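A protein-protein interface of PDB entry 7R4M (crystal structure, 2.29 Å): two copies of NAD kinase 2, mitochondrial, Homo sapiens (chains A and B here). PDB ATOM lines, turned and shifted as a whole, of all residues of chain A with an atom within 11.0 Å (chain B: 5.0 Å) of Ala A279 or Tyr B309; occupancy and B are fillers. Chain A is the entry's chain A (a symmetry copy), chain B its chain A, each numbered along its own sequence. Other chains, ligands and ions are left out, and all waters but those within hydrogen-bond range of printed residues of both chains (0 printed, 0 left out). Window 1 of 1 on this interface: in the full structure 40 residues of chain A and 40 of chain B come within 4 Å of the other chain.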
ATOM      1  N   ASN A 273      -7.624 -15.035  -2.296  1.00  0.00           N
ATOM      2  CA  ASN A 273      -8.632 -14.592  -1.343  1.00  0.00           C
ATOM      3  C   ASN A 273      -9.839 -13.906  -1.964  1.00  0.00           C
ATOM      4  O   ASN A 273     -10.890 -13.850  -1.318  1.00  0.00           O
ATOM      5  CB  ASN A 273      -8.002 -13.611  -0.340  1.00  0.00           C
ATOM      6  CG  ASN A 273      -7.083 -14.295   0.642  1.00  0.00           C
ATOM      7  OD1 ASN A 273      -7.519 -15.171   1.378  1.00  0.00           O
ATOM      8  ND2 ASN A 273      -5.799 -13.889   0.672  1.00  0.00           N
ATOM      9  N   ARG A 274      -9.705 -13.332  -3.158  1.00  0.00           N
ATOM     10  CA  ARG A 274     -10.807 -12.598  -3.767  1.00  0.00           C
ATOM     11  C   ARG A 274     -11.971 -13.540  -4.062  1.00  0.00           C
ATOM     12  O   ARG A 274     -11.788 -14.721  -4.376  1.00  0.00           O
ATOM     13  CB  ARG A 274     -10.346 -11.907  -5.058  1.00  0.00           C
ATOM     14  CG  ARG A 274      -9.912 -12.880  -6.168  1.00  0.00           C
ATOM     15  CD  ARG A 274      -9.159 -12.183  -7.295  1.00  0.00           C
ATOM     16  NE  ARG A 274     -10.038 -11.988  -8.436  1.00  0.00           N
ATOM     17  CZ  ARG A 274      -9.900 -12.592  -9.610  1.00  0.00           C
ATOM     18  NH1 ARG A 274      -8.859 -13.371  -9.872  1.00  0.00           N
ATOM     19  NH2 ARG A 274     -10.832 -12.408 -10.548  1.00  0.00           N
ATOM     20  N   VAL A 275     -13.176 -13.017  -3.933  1.00  0.00           N
ATOM     21  CA  VAL A 275     -14.377 -13.782  -4.244  1.00  0.00           C
ATOM     22  C   VAL A 275     -14.891 -13.351  -5.607  1.00  0.00           C
ATOM     23  O   VAL A 275     -14.719 -12.202  -6.038  1.00  0.00           O
ATOM     24  CB  VAL A 275     -15.469 -13.641  -3.162  1.00  0.00           C
ATOM     25  CG1 VAL A 275     -14.870 -13.799  -1.780  1.00  0.00           C
ATOM     26  CG2 VAL A 275     -16.130 -12.293  -3.282  1.00  0.00           C
ATOM     27  N   ALA A 276     -15.492 -14.307  -6.306  1.00  0.00           N
ATOM     28  CA  ALA A 276     -16.058 -14.068  -7.619  1.00  0.00           C
ATOM     29  C   ALA A 276     -17.387 -13.346  -7.485  1.00  0.00           C
ATOM     30  O   ALA A 276     -18.101 -13.485  -6.484  1.00  0.00           O
ATOM     31  CB  ALA A 276     -16.243 -15.391  -8.361  1.00  0.00           C
ATOM     32  N   THR A 277     -17.715 -12.558  -8.507  1.00  0.00           N
ATOM     33  CA  THR A 277     -18.982 -11.840  -8.488  1.00  0.00           C
ATOM     34  C   THR A 277     -20.164 -12.815  -8.498  1.00  0.00           C
ATOM     35  O   THR A 277     -21.228 -12.511  -7.943  1.00  0.00           O
ATOM     36  CB  THR A 277     -19.032 -10.844  -9.661  1.00  0.00           C
ATOM     37  OG1 THR A 277     -20.199 -10.020  -9.568  1.00  0.00           O
ATOM     38  CG2 THR A 277     -19.022 -11.564 -11.002  1.00  0.00           C
ATOM     39  N   GLN A 278     -19.982 -14.010  -9.066  1.00  0.00           N
ATOM     40  CA  GLN A 278     -21.034 -15.022  -9.003  1.00  0.00           C
ATOM     41  C   GLN A 278     -21.248 -15.502  -7.571  1.00  0.00           C
ATOM     42  O   GLN A 278     -22.393 -15.621  -7.112  1.00  0.00           O
ATOM     43  CB  GLN A 278     -20.693 -16.201  -9.918  1.00  0.00           C
ATOM     44  CG  GLN A 278     -21.745 -17.303  -9.937  1.00  0.00           C
ATOM     45  CD  GLN A 278     -23.145 -16.790 -10.264  1.00  0.00           C
ATOM     46  OE1 GLN A 278     -24.124 -17.199  -9.645  1.00  0.00           O
ATOM     47  NE2 GLN A 278     -23.243 -15.898 -11.242  1.00  0.00           N
ATOM     48  N   ALA A 279     -20.154 -15.780  -6.851  1.00  0.00           N
ATOM     49  CA  ALA A 279     -20.270 -16.237  -5.470  1.00  0.00           C
ATOM     50  C   ALA A 279     -20.999 -15.217  -4.612  1.00  0.00           C
ATOM     51  O   ALA A 279     -21.845 -15.585  -3.790  1.00  0.00           O
ATOM     52  CB  ALA A 279     -18.887 -16.538  -4.888  1.00  0.00           C
ATOM     53  N   VAL A 280     -20.691 -13.928  -4.800  1.00  0.00           N
ATOM     54  CA  VAL A 280     -21.414 -12.863  -4.106  1.00  0.00           C
ATOM     55  C   VAL A 280     -22.889 -12.878  -4.499  1.00  0.00           C
ATOM     56  O   VAL A 280     -23.781 -12.791  -3.644  1.00  0.00           O
ATOM     57  CB  VAL A 280     -20.770 -11.494  -4.405  1.00  0.00           C
ATOM     58  CG1 VAL A 280     -21.758 -10.367  -4.149  1.00  0.00           C
ATOM     59  CG2 VAL A 280     -19.514 -11.297  -3.575  1.00  0.00           C
ATOM     60  N   GLU A 281     -23.165 -12.975  -5.802  1.00  0.00           N
ATOM     61  CA  GLU A 281     -24.542 -13.083  -6.273  1.00  0.00           C
ATOM     62  C   GLU A 281     -25.267 -14.253  -5.617  1.00  0.00           C
ATOM     63  O   GLU A 281     -26.434 -14.128  -5.225  1.00  0.00           O
ATOM     64  CB  GLU A 281     -24.559 -13.237  -7.794  1.00  0.00           C
ATOM     65  CG  GLU A 281     -25.924 -13.074  -8.438  1.00  0.00           C
ATOM     66  CD  GLU A 281     -25.835 -12.931  -9.950  1.00  0.00           C
ATOM     67  OE1 GLU A 281     -24.798 -13.351 -10.515  1.00  0.00           O
ATOM     68  OE2 GLU A 281     -26.784 -12.390 -10.570  1.00  0.00           O
ATOM     69  N   ASP A 282     -24.592 -15.400  -5.490  1.00  0.00           N
ATOM     70  CA  ASP A 282     -25.201 -16.552  -4.833  1.00  0.00           C
ATOM     71  C   ASP A 282     -25.456 -16.273  -3.357  1.00  0.00           C
ATOM     72  O   ASP A 282     -26.573 -16.469  -2.867  1.00  0.00           O
ATOM     73  CB  ASP A 282     -24.309 -17.784  -4.999  1.00  0.00           C
ATOM     74  CG  ASP A 282     -24.300 -18.310  -6.421  1.00  0.00           C
ATOM     75  OD1 ASP A 282     -25.098 -17.794  -7.227  1.00  0.00           O
ATOM     76  OD2 ASP A 282     -23.511 -19.233  -6.729  1.00  0.00           O
ATOM     77  N   VAL A 283     -24.430 -15.807  -2.637  1.00  0.00           N
ATOM     78  CA  VAL A 283     -24.547 -15.535  -1.203  1.00  0.00           C
ATOM     79  C   VAL A 283     -25.706 -14.589  -0.919  1.00  0.00           C
ATOM     80  O   VAL A 283     -26.473 -14.785   0.034  1.00  0.00           O
ATOM     81  CB  VAL A 283     -23.215 -14.979  -0.661  1.00  0.00           C
ATOM     82  CG1 VAL A 283     -23.354 -14.527   0.786  1.00  0.00           C
ATOM     83  CG2 VAL A 283     -22.128 -16.032  -0.770  1.00  0.00           C
ATOM     84  N   LEU A 284     -25.864 -13.557  -1.754  1.00  0.00           N
ATOM     85  CA  LEU A 284     -26.962 -12.615  -1.573  1.00  0.00           C
ATOM     86  C   LEU A 284     -28.311 -13.280  -1.829  1.00  0.00           C
ATOM     87  O   LEU A 284     -29.271 -13.069  -1.078  1.00  0.00           O
ATOM     88  CB  LEU A 284     -26.757 -11.411  -2.493  1.00  0.00           C
ATOM     89  CG  LEU A 284     -25.544 -10.559  -2.115  1.00  0.00           C
ATOM     90  CD1 LEU A 284     -25.517  -9.257  -2.910  1.00  0.00           C
ATOM     91  CD2 LEU A 284     -25.557 -10.290  -0.614  1.00  0.00           C
ATOM     92  N   ASN A 285     -28.400 -14.096  -2.881  1.00  0.00           N
ATOM     93  CA  ASN A 285     -29.657 -14.771  -3.182  1.00  0.00           C
ATOM     94  C   ASN A 285     -30.040 -15.727  -2.061  1.00  0.00           C
ATOM     95  O   ASN A 285     -31.222 -15.869  -1.733  1.00  0.00           O
ATOM     96  CB  ASN A 285     -29.541 -15.507  -4.515  1.00  0.00           C
ATOM     97  CG  ASN A 285     -29.975 -14.650  -5.689  1.00  0.00           C
ATOM     98  OD1 ASN A 285     -30.962 -13.922  -5.609  1.00  0.00           O
ATOM     99  ND2 ASN A 285     -29.225 -14.722  -6.786  1.00  0.00           N
ATOM    100  N   ILE A 286     -29.046 -16.377  -1.453  1.00  0.00           N
ATOM    101  CA  ILE A 286     -29.298 -17.242  -0.303  1.00  0.00           C
ATOM    102  C   ILE A 286     -29.937 -16.446   0.825  1.00  0.00           C
ATOM    103  O   ILE A 286     -30.844 -16.927   1.515  1.00  0.00           O
ATOM    104  CB  ILE A 286     -27.985 -17.900   0.154  1.00  0.00           C
ATOM    105  CG1 ILE A 286     -27.401 -18.756  -0.974  1.00  0.00           C
ATOM    106  CG2 ILE A 286     -28.210 -18.726   1.419  1.00  0.00           C
ATOM    107  CD1 ILE A 286     -26.537 -19.895  -0.512  1.00  0.00           C
ATOM    108  N   ALA A 287     -29.475 -15.206   1.019  1.00  0.00           N
ATOM    109  CA  ALA A 287     -29.946 -14.385   2.128  1.00  0.00           C
ATOM    110  C   ALA A 287     -31.396 -13.952   1.942  1.00  0.00           C
ATOM    111  O   ALA A 287     -32.090 -13.664   2.924  1.00  0.00           O
ATOM    112  CB  ALA A 287     -29.036 -13.169   2.292  1.00  0.00           C
ATOM    113  N   ARG A 289     -33.891 -16.113   0.281  1.00  0.00           N
ATOM    114  CA  ARG A 289     -34.603 -17.332   0.661  1.00  0.00           C
ATOM    115  C   ARG A 289     -34.650 -17.520   2.170  1.00  0.00           C
ATOM    116  O   ARG A 289     -35.714 -17.764   2.754  1.00  0.00           O
ATOM    117  CB  ARG A 289     -33.936 -18.559   0.031  1.00  0.00           C
ATOM    118  N   GLN A 290     -33.505 -17.372   2.818  1.00  0.00           N
ATOM    119  CA  GLN A 290     -33.318 -17.798   4.201  1.00  0.00           C
ATOM    120  C   GLN A 290     -33.529 -16.652   5.182  1.00  0.00           C
ATOM    121  O   GLN A 290     -32.712 -16.411   6.072  1.00  0.00           O
ATOM    122  CB  GLN A 290     -31.932 -18.401   4.360  1.00  0.00           C
ATOM    123  CG  GLN A 290     -31.835 -19.363   5.492  1.00  0.00           C
ATOM    124  CD  GLN A 290     -30.439 -19.875   5.689  1.00  0.00           C
ATOM    125  OE1 GLN A 290     -29.716 -20.179   4.734  1.00  0.00           O
ATOM    126  NE2 GLN A 290     -30.028 -19.919   6.932  1.00  0.00           N
ATOM    127  N   LEU A 297     -31.399  -7.113  -5.539  1.00  0.00           N
ATOM    128  CA  LEU A 297     -30.122  -7.509  -6.116  1.00  0.00           C
ATOM    129  C   LEU A 297     -30.135  -7.269  -7.617  1.00  0.00           C
ATOM    130  O   LEU A 297     -31.020  -7.753  -8.328  1.00  0.00           O
ATOM    131  CB  LEU A 297     -29.828  -8.979  -5.814  1.00  0.00           C
ATOM    132  N   LEU A 301     -25.524  -3.720  -8.213  1.00  0.00           N
ATOM    133  CA  LEU A 301     -25.270  -3.895  -6.785  1.00  0.00           C
ATOM    134  C   LEU A 301     -24.288  -5.031  -6.525  1.00  0.00           C
ATOM    135  O   LEU A 301     -23.401  -4.911  -5.671  1.00  0.00           O
ATOM    136  CB  LEU A 301     -26.578  -4.146  -6.037  1.00  0.00           C
ATOM    137  CG  LEU A 301     -26.405  -4.913  -4.724  1.00  0.00           C
ATOM    138  CD1 LEU A 301     -25.951  -3.978  -3.611  1.00  0.00           C
ATOM    139  CD2 LEU A 301     -27.682  -5.611  -4.330  1.00  0.00           C
ATOM    140  N   VAL A 302     -24.427  -6.140  -7.255  1.00  0.00           N
ATOM    141  CA  VAL A 302     -23.587  -7.306  -6.999  1.00  0.00           C
ATOM    142  C   VAL A 302     -22.125  -6.991  -7.300  1.00  0.00           C
ATOM    143  O   VAL A 302     -21.230  -7.373  -6.537  1.00  0.00           O
ATOM    144  CB  VAL A 302     -24.103  -8.521  -7.795  1.00  0.00           C
ATOM    145  CG1 VAL A 302     -22.996  -9.540  -8.025  1.00  0.00           C
ATOM    146  CG2 VAL A 302     -25.264  -9.169  -7.063  1.00  0.00           C
ATOM    147  N   GLU A 303     -21.855  -6.288  -8.406  1.00  0.00           N
ATOM    148  CA  GLU A 303     -20.475  -5.883  -8.681  1.00  0.00           C
ATOM    149  C   GLU A 303     -19.928  -4.987  -7.580  1.00  0.00           C
ATOM    150  O   GLU A 303     -18.752  -5.093  -7.199  1.00  0.00           O
ATOM    151  CB  GLU A 303     -20.365  -5.159 -10.024  1.00  0.00           C
ATOM    152  CG  GLU A 303     -21.272  -5.676 -11.086  1.00  0.00           C
ATOM    153  CD  GLU A 303     -20.588  -5.756 -12.421  1.00  0.00           C
ATOM    154  OE1 GLU A 303     -19.490  -5.181 -12.561  1.00  0.00           O
ATOM    155  OE2 GLU A 303     -21.148  -6.388 -13.334  1.00  0.00           O
ATOM    156  N   VAL A 305     -20.862  -4.585  -4.258  1.00  0.00           N
ATOM    157  CA  VAL A 305     -20.544  -5.315  -3.028  1.00  0.00           C
ATOM    158  C   VAL A 305     -19.339  -6.226  -3.243  1.00  0.00           C
ATOM    159  O   VAL A 305     -18.499  -6.386  -2.348  1.00  0.00           O
ATOM    160  CB  VAL A 305     -21.767  -6.107  -2.517  1.00  0.00           C
ATOM    161  CG1 VAL A 305     -22.420  -6.871  -3.632  1.00  0.00           C
ATOM    162  CG2 VAL A 305     -21.360  -7.091  -1.412  1.00  0.00           C
ATOM    163  N   THR A 306     -19.219  -6.825  -4.431  1.00  0.00           N
ATOM    164  CA  THR A 306     -18.036  -7.640  -4.716  1.00  0.00           C
ATOM    165  C   THR A 306     -16.770  -6.805  -4.606  1.00  0.00           C
ATOM    166  O   THR A 306     -15.794  -7.208  -3.965  1.00  0.00           O
ATOM    167  CB  THR A 306     -18.121  -8.264  -6.114  1.00  0.00           C
ATOM    168  OG1 THR A 306     -19.411  -8.862  -6.322  1.00  0.00           O
ATOM    169  CG2 THR A 306     -17.027  -9.327  -6.285  1.00  0.00           C
ATOM    170  N   ASN A 307     -16.776  -5.633  -5.234  1.00  0.00           N
ATOM    171  CA  ASN A 307     -15.599  -4.776  -5.250  1.00  0.00           C
ATOM    172  C   ASN A 307     -15.257  -4.285  -3.852  1.00  0.00           C
ATOM    173  O   ASN A 307     -14.080  -4.169  -3.496  1.00  0.00           O
ATOM    174  CB  ASN A 307     -15.851  -3.605  -6.195  1.00  0.00           C
ATOM    175  CG  ASN A 307     -15.914  -4.035  -7.646  1.00  0.00           C
ATOM    176  OD1 ASN A 307     -15.685  -5.202  -7.966  1.00  0.00           O
ATOM    177  ND2 ASN A 307     -16.296  -3.111  -8.525  1.00  0.00           N
ATOM    178  N   TYR A 309     -15.759  -5.900  -1.060  1.00  0.00           N
ATOM    179  CA  TYR A 309     -15.119  -7.003  -0.354  1.00  0.00           C
ATOM    180  C   TYR A 309     -13.673  -7.168  -0.791  1.00  0.00           C
ATOM    181  O   TYR A 309     -12.795  -7.437   0.038  1.00  0.00           O
ATOM    182  CB  TYR A 309     -15.856  -8.322  -0.566  1.00  0.00           C
ATOM    183  CG  TYR A 309     -15.169  -9.412   0.225  1.00  0.00           C
ATOM    184  CD1 TYR A 309     -15.453  -9.589   1.570  1.00  0.00           C
ATOM    185  CD2 TYR A 309     -14.187 -10.221  -0.345  1.00  0.00           C
ATOM    186  CE1 TYR A 309     -14.816 -10.555   2.316  1.00  0.00           C
ATOM    187  CE2 TYR A 309     -13.546 -11.189   0.396  1.00  0.00           C
ATOM    188  CZ  TYR A 309     -13.866 -11.347   1.728  1.00  0.00           C
ATOM    189  OH  TYR A 309     -13.240 -12.293   2.497  1.00  0.00           O
ATOM    190  N   ASN A 310     -13.410  -7.045  -2.090  1.00  0.00           N
ATOM    191  CA  ASN A 310     -12.081  -7.371  -2.582  1.00  0.00           C
ATOM    192  C   ASN A 310     -11.069  -6.290  -2.231  1.00  0.00           C
ATOM    193  O   ASN A 310      -9.903  -6.611  -1.958  1.00  0.00           O
ATOM    194  CB  ASN A 310     -12.136  -7.631  -4.085  1.00  0.00           C
ATOM    195  CG  ASN A 310     -12.903  -8.912  -4.424  1.00  0.00           C
ATOM    196  OD1 ASN A 310     -12.889  -9.888  -3.661  1.00  0.00           O
ATOM    197  ND2 ASN A 310     -13.587  -8.906  -5.565  1.00  0.00           N
ATOM    198  N   ASN B 273     -12.930 -23.907  -3.397  1.00  0.00           N
ATOM    199  CA  ASN B 273     -14.108 -23.119  -3.731  1.00  0.00           C
ATOM    200  C   ASN B 273     -14.931 -22.662  -2.536  1.00  0.00           C
ATOM    201  O   ASN B 273     -15.691 -21.699  -2.670  1.00  0.00           O
ATOM    202  CB  ASN B 273     -15.032 -23.933  -4.651  1.00  0.00           C
ATOM    203  CG  ASN B 273     -14.482 -24.077  -6.048  1.00  0.00           C
ATOM    204  OD1 ASN B 273     -14.262 -23.080  -6.724  1.00  0.00           O
ATOM    205  ND2 ASN B 273     -14.267 -25.327  -6.502  1.00  0.00           N
ATOM    206  N   VAL B 275     -16.291 -20.907   0.761  1.00  0.00           N
ATOM    207  CA  VAL B 275     -16.067 -19.592   1.349  1.00  0.00           C
ATOM    208  C   VAL B 275     -16.084 -19.724   2.862  1.00  0.00           C
ATOM    209  O   VAL B 275     -16.761 -20.588   3.436  1.00  0.00           O
ATOM    210  CB  VAL B 275     -17.089 -18.542   0.865  1.00  0.00           C
ATOM    211  CG1 VAL B 275     -17.263 -18.624  -0.638  1.00  0.00           C
ATOM    212  CG2 VAL B 275     -18.412 -18.773   1.546  1.00  0.00           C
ATOM    213  N   VAL B 305     -26.273 -19.392   6.083  1.00  0.00           N
ATOM    214  CA  VAL B 305     -26.046 -18.969   4.699  1.00  0.00           C
ATOM    215  C   VAL B 305     -24.705 -19.491   4.194  1.00  0.00           C
ATOM    216  O   VAL B 305     -24.575 -19.878   3.025  1.00  0.00           O
ATOM    217  CB  VAL B 305     -26.142 -17.434   4.561  1.00  0.00           C
ATOM    218  CG1 VAL B 305     -25.356 -16.745   5.639  1.00  0.00           C
ATOM    219  CG2 VAL B 305     -25.621 -16.972   3.194  1.00  0.00           C
ATOM    220  N   THR B 306     -23.688 -19.532   5.061  1.00  0.00           N
ATOM    221  CA  THR B 306     -22.405 -20.105   4.648  1.00  0.00           C
ATOM    222  C   THR B 306     -22.576 -21.557   4.229  1.00  0.00           C
ATOM    223  O   THR B 306     -22.090 -21.977   3.174  1.00  0.00           O
ATOM    224  CB  THR B 306     -21.373 -20.015   5.779  1.00  0.00           C
ATOM    225  OG1 THR B 306     -21.364 -18.696   6.349  1.00  0.00           O
ATOM    226  CG2 THR B 306     -19.975 -20.355   5.245  1.00  0.00           C
ATOM    227  N   ASN B 307     -23.269 -22.336   5.054  1.00  0.00           N
ATOM    228  CA  ASN B 307     -23.445 -23.755   4.787  1.00  0.00           C
ATOM    229  C   ASN B 307     -24.260 -23.981   3.523  1.00  0.00           C
ATOM    230  O   ASN B 307     -23.989 -24.911   2.757  1.00  0.00           O
ATOM    231  CB  ASN B 307     -24.115 -24.408   5.993  1.00  0.00           C
ATOM    232  CG  ASN B 307     -23.208 -24.453   7.205  1.00  0.00           C
ATOM    233  OD1 ASN B 307     -22.040 -24.073   7.130  1.00  0.00           O
ATOM    234  ND2 ASN B 307     -23.763 -24.850   8.349  1.00  0.00           N
ATOM    235  N   GLU B 308     -25.258 -23.141   3.283  1.00  0.00           N
ATOM    236  CA  GLU B 308     -26.039 -23.303   2.064  1.00  0.00           C
ATOM    237  C   GLU B 308     -25.173 -23.069   0.836  1.00  0.00           C
ATOM    238  O   GLU B 308     -25.270 -23.804  -0.156  1.00  0.00           O
ATOM    239  CB  GLU B 308     -27.235 -22.354   2.074  1.00  0.00           C
ATOM    240  CG  GLU B 308     -28.190 -22.556   0.919  1.00  0.00           C
ATOM    241  CD  GLU B 308     -29.620 -22.358   1.336  1.00  0.00           C
ATOM    242  OE1 GLU B 308     -29.924 -22.568   2.526  1.00  0.00           O
ATOM    243  OE2 GLU B 308     -30.435 -21.976   0.477  1.00  0.00           O
ATOM    244  N   TYR B 309     -24.305 -22.058   0.885  1.00  0.00           N
ATOM    245  CA  TYR B 309     -23.426 -21.810  -0.250  1.00  0.00           C
ATOM    246  C   TYR B 309     -22.491 -22.985  -0.486  1.00  0.00           C
ATOM    247  O   TYR B 309     -22.231 -23.357  -1.637  1.00  0.00           O
ATOM    248  CB  TYR B 309     -22.595 -20.544  -0.064  1.00  0.00           C
ATOM    249  CG  TYR B 309     -21.740 -20.322  -1.292  1.00  0.00           C
ATOM    250  CD1 TYR B 309     -22.265 -19.690  -2.408  1.00  0.00           C
ATOM    251  CD2 TYR B 309     -20.433 -20.802  -1.369  1.00  0.00           C
ATOM    252  CE1 TYR B 309     -21.513 -19.505  -3.547  1.00  0.00           C
ATOM    253  CE2 TYR B 309     -19.676 -20.620  -2.505  1.00  0.00           C
ATOM    254  CZ  TYR B 309     -20.226 -19.973  -3.591  1.00  0.00           C
ATOM    255  OH  TYR B 309     -19.506 -19.785  -4.741  1.00  0.00           O
ATOM    256  N   ASN B 310     -21.951 -23.560   0.585  1.00  0.00           N
ATOM    257  CA  ASN B 310     -20.915 -24.565   0.408  1.00  0.00           C
ATOM    258  C   ASN B 310     -21.492 -25.892  -0.065  1.00  0.00           C
ATOM    259  O   ASN B 310     -20.840 -26.594  -0.852  1.00  0.00           O
ATOM    260  CB  ASN B 310     -20.121 -24.722   1.703  1.00  0.00           C
ATOM    261  CG  ASN B 310     -19.283 -23.481   2.021  1.00  0.00           C
ATOM    262  OD1 ASN B 310     -18.799 -22.786   1.117  1.00  0.00           O
ATOM    263  ND2 ASN B 310     -19.120 -23.193   3.311  1.00  0.00           N
ATOM    264  N   GLU B 311     -22.718 -26.224   0.349  1.00  0.00           N
ATOM    265  CA  GLU B 311     -23.387 -27.411  -0.178  1.00  0.00           C
ATOM    266  C   GLU B 311     -23.595 -27.312  -1.686  1.00  0.00           C
ATOM    267  O   GLU B 311     -23.527 -28.327  -2.393  1.00  0.00           O
ATOM    268  CB  GLU B 311     -24.729 -27.626   0.527  1.00  0.00           C
ATOM    269  CG  GLU B 311     -24.870 -28.987   1.214  1.00  0.00           C
ATOM    270  CD  GLU B 311     -24.974 -30.161   0.236  1.00  0.00           C
ATOM    271  OE1 GLU B 311     -25.128 -29.931  -0.986  1.00  0.00           O
ATOM    272  OE2 GLU B 311     -24.912 -31.329   0.691  1.00  0.00           O
ATOM    273  N   SER B 312     -23.821 -26.097  -2.202  1.00  0.00           N
ATOM    274  CA  SER B 312     -23.974 -25.923  -3.643  1.00  0.00           C
ATOM    275  C   SER B 312     -22.750 -26.396  -4.418  1.00  0.00           C
ATOM    276  O   SER B 312     -22.851 -26.633  -5.630  1.00  0.00           O
ATOM    277  CB  SER B 312     -24.276 -24.453  -3.965  1.00  0.00           C
ATOM    278  OG  SER B 312     -23.181 -23.585  -3.667  1.00  0.00           O
ATOM    279  N   LEU B 313     -21.604 -26.555  -3.744  1.00  0.00           N
ATOM    280  CA  LEU B 313     -20.383 -27.034  -4.381  1.00  0.00           C
ATOM    281  C   LEU B 313     -20.316 -28.549  -4.475  1.00  0.00           C
ATOM    282  O   LEU B 313     -19.486 -29.067  -5.226  1.00  0.00           O
ATOM    283  CB  LEU B 313     -19.168 -26.536  -3.612  1.00  0.00           C
ATOM    284  CG  LEU B 313     -19.008 -25.015  -3.506  1.00  0.00           C
ATOM    285  CD1 LEU B 313     -17.957 -24.663  -2.461  1.00  0.00           C
ATOM    286  CD2 LEU B 313     -18.653 -24.402  -4.861  1.00  0.00           C
ATOM    287  N   ARG B 341     -15.767 -21.235 -12.012  1.00  0.00           N
ATOM    288  CA  ARG B 341     -16.147 -22.637 -11.955  1.00  0.00           C
ATOM    289  C   ARG B 341     -17.471 -22.839 -12.685  1.00  0.00           C
ATOM    290  O   ARG B 341     -18.285 -21.918 -12.789  1.00  0.00           O
ATOM    291  CB  ARG B 341     -16.250 -23.128 -10.500  1.00  0.00           C
ATOM    292  CG  ARG B 341     -17.671 -23.364 -10.024  1.00  0.00           C
ATOM    293  CD  ARG B 341     -17.699 -23.828  -8.597  1.00  0.00           C
ATOM    294  NE  ARG B 341     -17.262 -22.742  -7.736  1.00  0.00           N
ATOM    295  CZ  ARG B 341     -18.086 -21.938  -7.084  1.00  0.00           C
ATOM    296  NH1 ARG B 341     -19.402 -22.104  -7.145  1.00  0.00           N
ATOM    297  NH2 ARG B 341     -17.577 -20.946  -6.355  1.00  0.00           N
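The side-chain carboxylate (OE1) of Glu B308 sits close to the side-chain amide oxygen (OE1) of Gln A290, at 3.3 Å.
The guanidinium group (NH2) of Arg B341 is in hydrogen-bond range of the side-chain hydroxyl (OH) of Tyr B309, 2.8 Å away.
The side-chain carboxylate (OD1) of Asp A282 lies close to the side-chain amide oxygen (OE1) of Gln A278, 2.7 Å away.
CB of Ala A279 touches OH of Tyr B309, 3.3 Å away.
Asp A282 touches Tyr B309 (CB to CE1, 3.6 Å).
O of Val A283 touches CG2 of Val B305 (3.9 Å).
Ile A286 touches Val B305 (CG2 to CG2, 3.6 Å).
Glu B308 touches Ile A286 (CG to CD1, 3.4 Å).
Ile A286 touches Tyr B309 (CD1 to N, 3.4 Å).
N of Val B305 touches OE1 of Gln A290 (3.8 Å).
Printed residues of chain B within 4 Å of Ala A279: Tyr B309.
No residue of chain A comes within 4 Å of Thr B306.
Of chain A, only Ile A286 and Gln A290 come within 4 Å of Glu B308.
No residue of chain A comes within 4 Å of Asn B310.
No residue of chain A comes within 4 Å of Ser B312.
Printed residues of chain B within 4 Å of Val A283: Val B305.
Printed residues of chain A within 4 Å of Val B305: Val A283, Ile A286 and Gln A290.
Printed residues of chain B within 4 Å of Ile A286: Val B305 (3.6 Å), Glu B308 (3.4 Å) and Tyr B309 (3.4 Å).
Of the printed residues of chain B, Gln A290 touches Val B305 and Glu B308.
Of the printed residues of chain B, Asp A282 touches Tyr B309.
The nearest printed residue of chain A that does not touch Tyr B309 is Val A283 (4.01 Å).
The nearest printed residue of chain A that does not touch Val B305 is Ala A287 (4.8 Å).
Printed residues of chain B that touch a printed residue of chain A: Val B305, Glu B308 and Tyr B309.
Of the 26 printed residues of chain A, 5 touch a printed residue of chain B.
Among the printed residues, no Asp or Glu carboxylate lies within 4 Å of a Lys or Arg side-chain nitrogen of the other chain.
7 positions are printed for both chains.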
